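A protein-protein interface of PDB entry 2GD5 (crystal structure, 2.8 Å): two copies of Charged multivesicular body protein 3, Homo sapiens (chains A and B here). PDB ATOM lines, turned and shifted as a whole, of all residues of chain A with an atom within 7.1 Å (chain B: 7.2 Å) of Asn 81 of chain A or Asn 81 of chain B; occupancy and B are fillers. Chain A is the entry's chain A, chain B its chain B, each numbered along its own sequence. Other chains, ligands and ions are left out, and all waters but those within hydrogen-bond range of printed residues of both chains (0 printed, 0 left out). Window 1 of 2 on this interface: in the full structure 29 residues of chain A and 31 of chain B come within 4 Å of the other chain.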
ATOM      1  N   ILE A  19      -6.269  22.290   8.606  1.00  0.00           N
ATOM      2  CA  ILE A  19      -7.654  22.344   9.051  1.00  0.00           C
ATOM      3  C   ILE A  19      -8.354  21.046   8.703  1.00  0.00           C
ATOM      4  O   ILE A  19      -8.957  20.409   9.588  1.00  0.00           O
ATOM      5  CB  ILE A  19      -8.433  23.522   8.441  1.00  0.00           C
ATOM      6  CG1 ILE A  19      -8.032  24.822   9.121  1.00  0.00           C
ATOM      7  CG2 ILE A  19      -9.926  23.297   8.579  1.00  0.00           C
ATOM      8  CD1 ILE A  19      -8.142  24.776  10.609  1.00  0.00           C
ATOM      9  N   ARG A  20      -8.264  20.648   7.435  1.00  0.00           N
ATOM     10  CA  ARG A  20      -8.872  19.422   6.978  1.00  0.00           C
ATOM     11  C   ARG A  20      -8.311  18.268   7.786  1.00  0.00           C
ATOM     12  O   ARG A  20      -9.028  17.307   8.053  1.00  0.00           O
ATOM     13  CB  ARG A  20      -8.598  19.224   5.494  1.00  0.00           C
ATOM     14  CG  ARG A  20      -9.426  18.157   4.809  1.00  0.00           C
ATOM     15  CD  ARG A  20     -10.809  18.680   4.416  1.00  0.00           C
ATOM     16  NE  ARG A  20     -11.655  17.623   3.849  1.00  0.00           N
ATOM     17  CZ  ARG A  20     -12.368  16.754   4.564  1.00  0.00           C
ATOM     18  NH1 ARG A  20     -12.349  16.797   5.900  1.00  0.00           N
ATOM     19  NH2 ARG A  20     -13.107  15.833   3.947  1.00  0.00           N
ATOM     20  N   MET A  23      -9.917  18.185  11.111  1.00  0.00           N
ATOM     21  CA  MET A  23     -11.268  17.664  11.003  1.00  0.00           C
ATOM     22  C   MET A  23     -11.315  16.157  10.922  1.00  0.00           C
ATOM     23  O   MET A  23     -12.239  15.563  11.415  1.00  0.00           O
ATOM     24  CB  MET A  23     -12.004  18.282   9.844  1.00  0.00           C
ATOM     25  CG  MET A  23     -12.219  19.782  10.003  1.00  0.00           C
ATOM     26  SD  MET A  23     -12.913  20.627   8.391  1.00  0.00           S
ATOM     27  CE  MET A  23     -14.469  19.450   8.128  1.00  0.00           C
ATOM     28  N   ALA A  75     -19.463  21.057  17.297  1.00  0.00           N
ATOM     29  CA  ALA A  75     -19.268  22.511  17.304  1.00  0.00           C
ATOM     30  C   ALA A  75     -17.942  22.800  16.559  1.00  0.00           C
ATOM     31  O   ALA A  75     -17.933  23.466  15.529  1.00  0.00           O
ATOM     32  CB  ALA A  75     -19.228  23.047  18.701  1.00  0.00           C
ATOM     33  N   SER A  76     -16.847  22.235  17.060  1.00  0.00           N
ATOM     34  CA  SER A  76     -15.542  22.394  16.472  1.00  0.00           C
ATOM     35  C   SER A  76     -15.545  22.120  14.969  1.00  0.00           C
ATOM     36  O   SER A  76     -15.018  22.921  14.186  1.00  0.00           O
ATOM     37  CB  SER A  76     -14.576  21.451  17.149  1.00  0.00           C
ATOM     38  OG  SER A  76     -13.929  22.081  18.222  1.00  0.00           O
ATOM     39  N   LYS A  77     -16.133  21.004  14.549  1.00  0.00           N
ATOM     40  CA  LYS A  77     -16.065  20.679  13.140  1.00  0.00           C
ATOM     41  C   LYS A  77     -16.610  21.862  12.409  1.00  0.00           C
ATOM     42  O   LYS A  77     -15.982  22.311  11.460  1.00  0.00           O
ATOM     43  CB  LYS A  77     -16.847  19.436  12.778  1.00  0.00           C
ATOM     44  CG  LYS A  77     -16.380  18.737  11.528  1.00  0.00           C
ATOM     45  CD  LYS A  77     -17.172  17.449  11.371  1.00  0.00           C
ATOM     46  CE  LYS A  77     -16.993  16.734  10.028  1.00  0.00           C
ATOM     47  NZ  LYS A  77     -18.160  15.766   9.777  1.00  0.00           N
ATOM     48  N   ALA A  78     -17.757  22.386  12.848  1.00  0.00           N
ATOM     49  CA  ALA A  78     -18.356  23.576  12.226  1.00  0.00           C
ATOM     50  C   ALA A  78     -17.413  24.773  12.221  1.00  0.00           C
ATOM     51  O   ALA A  78     -17.158  25.350  11.158  1.00  0.00           O
ATOM     52  CB  ALA A  78     -19.657  23.936  12.899  1.00  0.00           C
ATOM     53  N   HIS A  79     -16.881  25.152  13.384  1.00  0.00           N
ATOM     54  CA  HIS A  79     -15.926  26.257  13.425  1.00  0.00           C
ATOM     55  C   HIS A  79     -14.808  26.028  12.393  1.00  0.00           C
ATOM     56  O   HIS A  79     -14.416  26.939  11.688  1.00  0.00           O
ATOM     57  CB  HIS A  79     -15.318  26.456  14.819  1.00  0.00           C
ATOM     58  CG  HIS A  79     -16.312  26.822  15.880  1.00  0.00           C
ATOM     59  ND1 HIS A  79     -16.952  28.045  15.918  1.00  0.00           N
ATOM     60  CD2 HIS A  79     -16.764  26.131  16.957  1.00  0.00           C
ATOM     61  CE1 HIS A  79     -17.766  28.085  16.960  1.00  0.00           C
ATOM     62  NE2 HIS A  79     -17.674  26.936  17.605  1.00  0.00           N
ATOM     63  N   MET A  80     -14.289  24.807  12.310  1.00  0.00           N
ATOM     64  CA  MET A  80     -13.237  24.508  11.351  1.00  0.00           C
ATOM     65  C   MET A  80     -13.767  24.693   9.929  1.00  0.00           C
ATOM     66  O   MET A  80     -13.099  25.312   9.088  1.00  0.00           O
ATOM     67  CB  MET A  80     -12.690  23.091  11.541  1.00  0.00           C
ATOM     68  CG  MET A  80     -11.876  22.934  12.787  1.00  0.00           C
ATOM     69  SD  MET A  80     -11.306  21.122  13.187  1.00  0.00           S
ATOM     70  CE  MET A  80     -12.828  20.309  13.154  1.00  0.00           C
ATOM     71  N   ASN A  81     -14.964  24.190   9.655  1.00  0.00           N
ATOM     72  CA  ASN A  81     -15.499  24.312   8.330  1.00  0.00           C
ATOM     73  C   ASN A  81     -15.631  25.759   7.995  1.00  0.00           C
ATOM     74  O   ASN A  81     -15.394  26.180   6.869  1.00  0.00           O
ATOM     75  CB  ASN A  81     -16.843  23.638   8.214  1.00  0.00           C
ATOM     76  CG  ASN A  81     -16.872  22.663   7.062  1.00  0.00           C
ATOM     77  OD1 ASN A  81     -16.555  23.029   5.932  1.00  0.00           O
ATOM     78  ND2 ASN A  81     -17.213  21.397   7.342  1.00  0.00           N
ATOM     79  N   SER A  82     -15.994  26.546   8.988  1.00  0.00           N
ATOM     80  CA  SER A  82     -16.098  27.976   8.780  1.00  0.00           C
ATOM     81  C   SER A  82     -14.745  28.475   8.262  1.00  0.00           C
ATOM     82  O   SER A  82     -14.680  29.170   7.244  1.00  0.00           O
ATOM     83  CB  SER A  82     -16.518  28.654  10.084  1.00  0.00           C
ATOM     84  OG  SER A  82     -16.489  30.054   9.978  1.00  0.00           O
ATOM     85  N   VAL A  83     -13.663  28.065   8.917  1.00  0.00           N
ATOM     86  CA  VAL A  83     -12.325  28.444   8.481  1.00  0.00           C
ATOM     87  C   VAL A  83     -11.967  27.959   7.080  1.00  0.00           C
ATOM     88  O   VAL A  83     -11.391  28.705   6.314  1.00  0.00           O
ATOM     89  CB  VAL A  83     -11.254  27.989   9.459  1.00  0.00           C
ATOM     90  CG1 VAL A  83      -9.874  28.167   8.840  1.00  0.00           C
ATOM     91  CG2 VAL A  83     -11.365  28.792  10.733  1.00  0.00           C
ATOM     92  N   LEU A  84     -12.295  26.717   6.750  1.00  0.00           N
ATOM     93  CA  LEU A  84     -12.015  26.210   5.428  1.00  0.00           C
ATOM     94  C   LEU A  84     -12.660  27.087   4.380  1.00  0.00           C
ATOM     95  O   LEU A  84     -12.003  27.519   3.458  1.00  0.00           O
ATOM     96  CB  LEU A  84     -12.553  24.815   5.294  1.00  0.00           C
ATOM     97  CG  LEU A  84     -11.625  23.874   4.562  1.00  0.00           C
ATOM     98  CD1 LEU A  84     -10.196  24.207   4.940  1.00  0.00           C
ATOM     99  CD2 LEU A  84     -11.941  22.420   4.907  1.00  0.00           C
ATOM    100  N   MET A  85     -13.954  27.361   4.545  1.00  0.00           N
ATOM    101  CA  MET A  85     -14.693  28.262   3.669  1.00  0.00           C
ATOM    102  C   MET A  85     -13.945  29.578   3.508  1.00  0.00           C
ATOM    103  O   MET A  85     -13.560  29.939   2.407  1.00  0.00           O
ATOM    104  CB  MET A  85     -16.069  28.544   4.233  1.00  0.00           C
ATOM    105  CG  MET A  85     -17.054  27.379   4.193  1.00  0.00           C
ATOM    106  SD  MET A  85     -17.178  26.575   2.461  1.00  0.00           S
ATOM    107  CE  MET A  85     -16.342  24.870   2.836  1.00  0.00           C
ATOM    108  N   GLY A  86     -13.721  30.293   4.603  1.00  0.00           N
ATOM    109  CA  GLY A  86     -12.854  31.476   4.563  1.00  0.00           C
ATOM    110  C   GLY A  86     -11.615  31.261   3.716  1.00  0.00           C
ATOM    111  O   GLY A  86     -11.301  32.108   2.888  1.00  0.00           O
ATOM    112  N   MET A  87     -10.923  30.130   3.900  1.00  0.00           N
ATOM    113  CA  MET A  87      -9.767  29.762   3.053  1.00  0.00           C
ATOM    114  C   MET A  87     -10.141  29.734   1.559  1.00  0.00           C
ATOM    115  O   MET A  87      -9.439  30.309   0.715  1.00  0.00           O
ATOM    116  CB  MET A  87      -9.161  28.416   3.469  1.00  0.00           C
ATOM    117  CG  MET A  87      -8.439  28.409   4.791  1.00  0.00           C
ATOM    118  SD  MET A  87      -7.365  29.937   4.812  1.00  0.00           S
ATOM    119  CE  MET A  87      -8.371  31.178   5.799  1.00  0.00           C
ATOM    120  N   ALA A 109     -13.691  32.299  14.429  1.00  0.00           N
ATOM    121  CA  ALA A 109     -13.717  30.847  14.329  1.00  0.00           C
ATOM    122  C   ALA A 109     -12.388  30.322  14.813  1.00  0.00           C
ATOM    123  O   ALA A 109     -12.325  29.349  15.551  1.00  0.00           O
ATOM    124  CB  ALA A 109     -13.961  30.408  12.890  1.00  0.00           C
ATOM    125  N   LEU A 113     -11.695  28.097  18.559  1.00  0.00           N
ATOM    126  CA  LEU A 113     -11.046  26.841  18.227  1.00  0.00           C
ATOM    127  C   LEU A 113      -9.763  26.669  19.029  1.00  0.00           C
ATOM    128  O   LEU A 113      -9.424  25.561  19.415  1.00  0.00           O
ATOM    129  CB  LEU A 113     -10.757  26.799  16.728  1.00  0.00           C
ATOM    130  CG  LEU A 113     -11.268  25.609  15.919  1.00  0.00           C
ATOM    131  CD1 LEU A 113     -12.374  24.832  16.642  1.00  0.00           C
ATOM    132  CD2 LEU A 113     -11.744  26.110  14.557  1.00  0.00           C
ATOM    133  N   ILE B  19     -31.628  22.313   3.793  1.00  0.00           N
ATOM    134  CA  ILE B  19     -30.433  23.086   4.138  1.00  0.00           C
ATOM    135  C   ILE B  19     -29.407  22.854   3.062  1.00  0.00           C
ATOM    136  O   ILE B  19     -28.676  23.775   2.664  1.00  0.00           O
ATOM    137  CB  ILE B  19     -29.828  22.644   5.502  1.00  0.00           C
ATOM    138  CG1 ILE B  19     -30.648  23.149   6.681  1.00  0.00           C
ATOM    139  CG2 ILE B  19     -28.371  23.109   5.677  1.00  0.00           C
ATOM    140  CD1 ILE B  19     -30.773  24.694   6.739  1.00  0.00           C
ATOM    141  N   ARG B  20     -29.350  21.613   2.593  1.00  0.00           N
ATOM    142  CA  ARG B  20     -28.370  21.228   1.614  1.00  0.00           C
ATOM    143  C   ARG B  20     -28.752  21.967   0.337  1.00  0.00           C
ATOM    144  O   ARG B  20     -27.914  22.670  -0.232  1.00  0.00           O
ATOM    145  CB  ARG B  20     -28.351  19.704   1.493  1.00  0.00           C
ATOM    146  CG  ARG B  20     -27.173  19.066   0.785  1.00  0.00           C
ATOM    147  CD  ARG B  20     -25.829  19.287   1.482  1.00  0.00           C
ATOM    148  NE  ARG B  20     -24.676  18.880   0.652  1.00  0.00           N
ATOM    149  CZ  ARG B  20     -23.980  19.667  -0.175  1.00  0.00           C
ATOM    150  NH1 ARG B  20     -24.269  20.955  -0.339  1.00  0.00           N
ATOM    151  NH2 ARG B  20     -22.972  19.151  -0.857  1.00  0.00           N
ATOM    152  N   MET B  23     -27.840  25.463   0.169  1.00  0.00           N
ATOM    153  CA  MET B  23     -26.416  25.651   0.089  1.00  0.00           C
ATOM    154  C   MET B  23     -25.977  25.582  -1.368  1.00  0.00           C
ATOM    155  O   MET B  23     -25.024  26.274  -1.760  1.00  0.00           O
ATOM    156  CB  MET B  23     -25.669  24.604   0.934  1.00  0.00           C
ATOM    157  CG  MET B  23     -25.833  24.767   2.502  1.00  0.00           C
ATOM    158  SD  MET B  23     -24.844  23.459   3.559  1.00  0.00           S
ATOM    159  CE  MET B  23     -23.153  23.732   2.770  1.00  0.00           C
ATOM    160  N   ALA B  75     -20.408  33.471   4.578  1.00  0.00           N
ATOM    161  CA  ALA B  75     -20.821  33.522   5.954  1.00  0.00           C
ATOM    162  C   ALA B  75     -22.023  32.583   6.063  1.00  0.00           C
ATOM    163  O   ALA B  75     -21.909  31.460   6.583  1.00  0.00           O
ATOM    164  CB  ALA B  75     -21.199  34.946   6.343  1.00  0.00           C
ATOM    165  N   SER B  76     -23.162  33.036   5.543  1.00  0.00           N
ATOM    166  CA  SER B  76     -24.359  32.209   5.448  1.00  0.00           C
ATOM    167  C   SER B  76     -24.059  30.735   5.220  1.00  0.00           C
ATOM    168  O   SER B  76     -24.656  29.899   5.873  1.00  0.00           O
ATOM    169  CB  SER B  76     -25.270  32.704   4.326  1.00  0.00           C
ATOM    170  OG  SER B  76     -26.172  33.697   4.787  1.00  0.00           O
ATOM    171  N   LYS B  77     -23.145  30.401   4.312  1.00  0.00           N
ATOM    172  CA  LYS B  77     -22.895  28.990   4.034  1.00  0.00           C
ATOM    173  C   LYS B  77     -22.321  28.283   5.262  1.00  0.00           C
ATOM    174  O   LYS B  77     -22.726  27.158   5.577  1.00  0.00           O
ATOM    175  CB  LYS B  77     -21.989  28.807   2.822  1.00  0.00           C
ATOM    176  CG  LYS B  77     -21.786  27.344   2.387  1.00  0.00           C
ATOM    177  CD  LYS B  77     -20.727  27.244   1.278  1.00  0.00           C
ATOM    178  CE  LYS B  77     -20.709  25.878   0.588  1.00  0.00           C
ATOM    179  NZ  LYS B  77     -19.678  25.894  -0.493  1.00  0.00           N
ATOM    180  N   ALA B  78     -21.387  28.945   5.952  1.00  0.00           N
ATOM    181  CA  ALA B  78     -20.861  28.447   7.217  1.00  0.00           C
ATOM    182  C   ALA B  78     -22.020  28.130   8.164  1.00  0.00           C
ATOM    183  O   ALA B  78     -22.160  26.973   8.599  1.00  0.00           O
ATOM    184  CB  ALA B  78     -19.919  29.456   7.839  1.00  0.00           C
ATOM    185  N   HIS B  79     -22.850  29.141   8.443  1.00  0.00           N
ATOM    186  CA  HIS B  79     -24.084  28.980   9.224  1.00  0.00           C
ATOM    187  C   HIS B  79     -24.885  27.762   8.813  1.00  0.00           C
ATOM    188  O   HIS B  79     -25.211  26.900   9.644  1.00  0.00           O
ATOM    189  CB  HIS B  79     -24.977  30.215   9.122  1.00  0.00           C
ATOM    190  CG  HIS B  79     -24.346  31.460   9.673  1.00  0.00           C
ATOM    191  ND1 HIS B  79     -23.611  31.472  10.849  1.00  0.00           N
ATOM    192  CD2 HIS B  79     -24.341  32.736   9.208  1.00  0.00           C
ATOM    193  CE1 HIS B  79     -23.189  32.699  11.088  1.00  0.00           C
ATOM    194  NE2 HIS B  79     -23.620  33.485  10.112  1.00  0.00           N
ATOM    195  N   MET B  80     -25.195  27.674   7.526  1.00  0.00           N
ATOM    196  CA  MET B  80     -25.899  26.525   7.038  1.00  0.00           C
ATOM    197  C   MET B  80     -25.126  25.270   7.427  1.00  0.00           C
ATOM    198  O   MET B  80     -25.726  24.340   7.976  1.00  0.00           O
ATOM    199  CB  MET B  80     -26.118  26.628   5.533  1.00  0.00           C
ATOM    200  CG  MET B  80     -27.153  27.670   5.186  1.00  0.00           C
ATOM    201  SD  MET B  80     -27.570  27.827   3.336  1.00  0.00           S
ATOM    202  CE  MET B  80     -26.009  28.508   2.764  1.00  0.00           C
ATOM    203  N   ASN B  81     -23.805  25.252   7.200  1.00  0.00           N
ATOM    204  CA  ASN B  81     -23.021  24.063   7.523  1.00  0.00           C
ATOM    205  C   ASN B  81     -23.120  23.750   9.008  1.00  0.00           C
ATOM    206  O   ASN B  81     -23.152  22.585   9.410  1.00  0.00           O
ATOM    207  CB  ASN B  81     -21.558  24.177   7.114  1.00  0.00           C
ATOM    208  CG  ASN B  81     -21.056  22.926   6.332  1.00  0.00           C
ATOM    209  OD1 ASN B  81     -21.665  21.858   6.364  1.00  0.00           O
ATOM    210  ND2 ASN B  81     -19.938  23.087   5.608  1.00  0.00           N
ATOM    211  N   SER B  82     -23.209  24.784   9.829  1.00  0.00           N
ATOM    212  CA  SER B  82     -23.374  24.561  11.247  1.00  0.00           C
ATOM    213  C   SER B  82     -24.710  23.824  11.498  1.00  0.00           C
ATOM    214  O   SER B  82     -24.760  22.864  12.294  1.00  0.00           O
ATOM    215  CB  SER B  82     -23.290  25.891  11.985  1.00  0.00           C
ATOM    216  OG  SER B  82     -23.490  25.725  13.363  1.00  0.00           O
ATOM    217  N   VAL B  83     -25.775  24.217  10.788  1.00  0.00           N
ATOM    218  CA  VAL B  83     -27.078  23.556  10.974  1.00  0.00           C
ATOM    219  C   VAL B  83     -27.001  22.153  10.467  1.00  0.00           C
ATOM    220  O   VAL B  83     -27.576  21.236  11.069  1.00  0.00           O
ATOM    221  CB  VAL B  83     -28.239  24.289  10.312  1.00  0.00           C
ATOM    222  CG1 VAL B  83     -29.452  23.447  10.310  1.00  0.00           C
ATOM    223  CG2 VAL B  83     -28.568  25.522  11.097  1.00  0.00           C
ATOM    224  N   LEU B  84     -26.274  21.945   9.384  1.00  0.00           N
ATOM    225  CA  LEU B  84     -26.179  20.594   8.905  1.00  0.00           C
ATOM    226  C   LEU B  84     -25.493  19.702   9.948  1.00  0.00           C
ATOM    227  O   LEU B  84     -25.965  18.590  10.184  1.00  0.00           O
ATOM    228  CB  LEU B  84     -25.488  20.542   7.557  1.00  0.00           C
ATOM    229  CG  LEU B  84     -25.716  19.371   6.591  1.00  0.00           C
ATOM    230  CD1 LEU B  84     -27.145  18.951   6.448  1.00  0.00           C
ATOM    231  CD2 LEU B  84     -25.216  19.802   5.231  1.00  0.00           C
ATOM    232  N   MET B  85     -24.426  20.185  10.595  1.00  0.00           N
ATOM    233  CA  MET B  85     -23.710  19.352  11.518  1.00  0.00           C
ATOM    234  C   MET B  85     -24.647  19.094  12.697  1.00  0.00           C
ATOM    235  O   MET B  85     -24.814  17.963  13.177  1.00  0.00           O
ATOM    236  CB  MET B  85     -22.460  20.047  12.033  1.00  0.00           C
ATOM    237  CG  MET B  85     -21.199  20.118  11.137  1.00  0.00           C
ATOM    238  SD  MET B  85     -20.907  18.490  10.208  1.00  0.00           S
ATOM    239  CE  MET B  85     -21.476  19.008   8.442  1.00  0.00           C
ATOM    240  N   GLY B  86     -25.288  20.145  13.167  1.00  0.00           N
ATOM    241  CA  GLY B  86     -26.276  19.967  14.217  1.00  0.00           C
ATOM    242  C   GLY B  86     -27.259  18.855  13.917  1.00  0.00           C
ATOM    243  O   GLY B  86     -27.645  18.136  14.836  1.00  0.00           O
ATOM    244  N   MET B  87     -27.665  18.702  12.648  1.00  0.00           N
ATOM    245  CA  MET B  87     -28.585  17.644  12.275  1.00  0.00           C
ATOM    246  C   MET B  87     -27.905  16.288  12.403  1.00  0.00           C
ATOM    247  O   MET B  87     -28.521  15.294  12.842  1.00  0.00           O
ATOM    248  CB  MET B  87     -29.135  17.820  10.826  1.00  0.00           C
ATOM    249  CG  MET B  87     -30.100  19.046  10.541  1.00  0.00           C
ATOM    250  SD  MET B  87     -31.372  19.321  11.961  1.00  0.00           S
ATOM    251  CE  MET B  87     -30.656  20.802  12.843  1.00  0.00           C
ATOM    252  N   ALA B 109     -27.329  29.772  14.595  1.00  0.00           N
ATOM    253  CA  ALA B 109     -27.073  29.736  13.164  1.00  0.00           C
ATOM    254  C   ALA B 109     -28.378  30.019  12.427  1.00  0.00           C
ATOM    255  O   ALA B 109     -28.411  30.827  11.498  1.00  0.00           O
ATOM    256  CB  ALA B 109     -26.509  28.400  12.754  1.00  0.00           C
ATOM    257  N   LEU B 113     -29.377  33.301  10.412  1.00  0.00           N
ATOM    258  CA  LEU B 113     -29.621  32.806   9.045  1.00  0.00           C
ATOM    259  C   LEU B 113     -30.911  33.304   8.452  1.00  0.00           C
ATOM    260  O   LEU B 113     -31.024  33.421   7.228  1.00  0.00           O
ATOM    261  CB  LEU B 113     -29.620  31.284   8.998  1.00  0.00           C
ATOM    262  CG  LEU B 113     -29.082  30.629   7.734  1.00  0.00           C
ATOM    263  CD1 LEU B 113     -27.996  31.467   7.103  1.00  0.00           C
ATOM    264  CD2 LEU B 113     -28.559  29.245   8.057  1.00  0.00           C
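OD1 of Asn 81 of chain A lies within hydrogen-bond range of ND2 of Asn 81 of chain B (3.4 Å).
SD of Met 85 of chain B touches NZ of Lys 77 of chain A, 3.9 Å away. Lys 77 of chain B touches Met 85 of chain A (CD to SD, 3.8 Å).
Ile 19 of chain A touches none of the printed residues of chain B. Of the printed residues of chain B, Lys 77 of chain A touches Met 85. Of chain B, only Asn 81 (3.4 Å) comes within 4 Å of Asn 81 of chain A. Of the printed residues of chain B, Met 85 of chain A touches Lys 77 (3.8 Å). Printed residues of chain A within 4 Å of Lys 77 of chain B: Met 85 (3.8 Å). Of chain A, only Asn 81 (3.4 Å) comes within 4 Å of Asn 81 of chain B. The nearest residue of chain A that does not touch Asn 81 of chain B is Met 85 of chain A (4.9 Å). The nearest printed residue of chain B that does not touch Lys 77 of chain A is Asn 81 of chain B (7.1 Å).
Of the 18 printed residues of chain B, 3 touch a printed residue of chain A. Hydrophobic or aromatic side chains of chain B within 4 Å of the printed part of chain A: Met 85. Of the 18 printed residues of chain A, 3 touch a printed residue of chain B. Printed residues of chain A that touch a printed residue of chain B: Lys 77, Asn 81 and Met 85. Hydrophobic or aromatic side chains of chain A within 4 Å of the printed part of chain B: Met 85. Among the printed residues, 3 pairs touch across the chains.
Lys 77 of chain A touches Met 85 of chain B, and with the chains exchanged Met 85 of chain A touches Lys 77 of chain B. Asn 81 of chain A touches its own counterpart, Asn 81 of chain B. Positions printed for both chains: 19, 20, 23, 75, 76, 77, 78, 79, 80, 81, 82, 83, 84, 85, 86, 87, 109 and 113. Of the 3 pairs that touch across the chains among the printed residues, 3 have their exchanged pair printed and touching as well.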
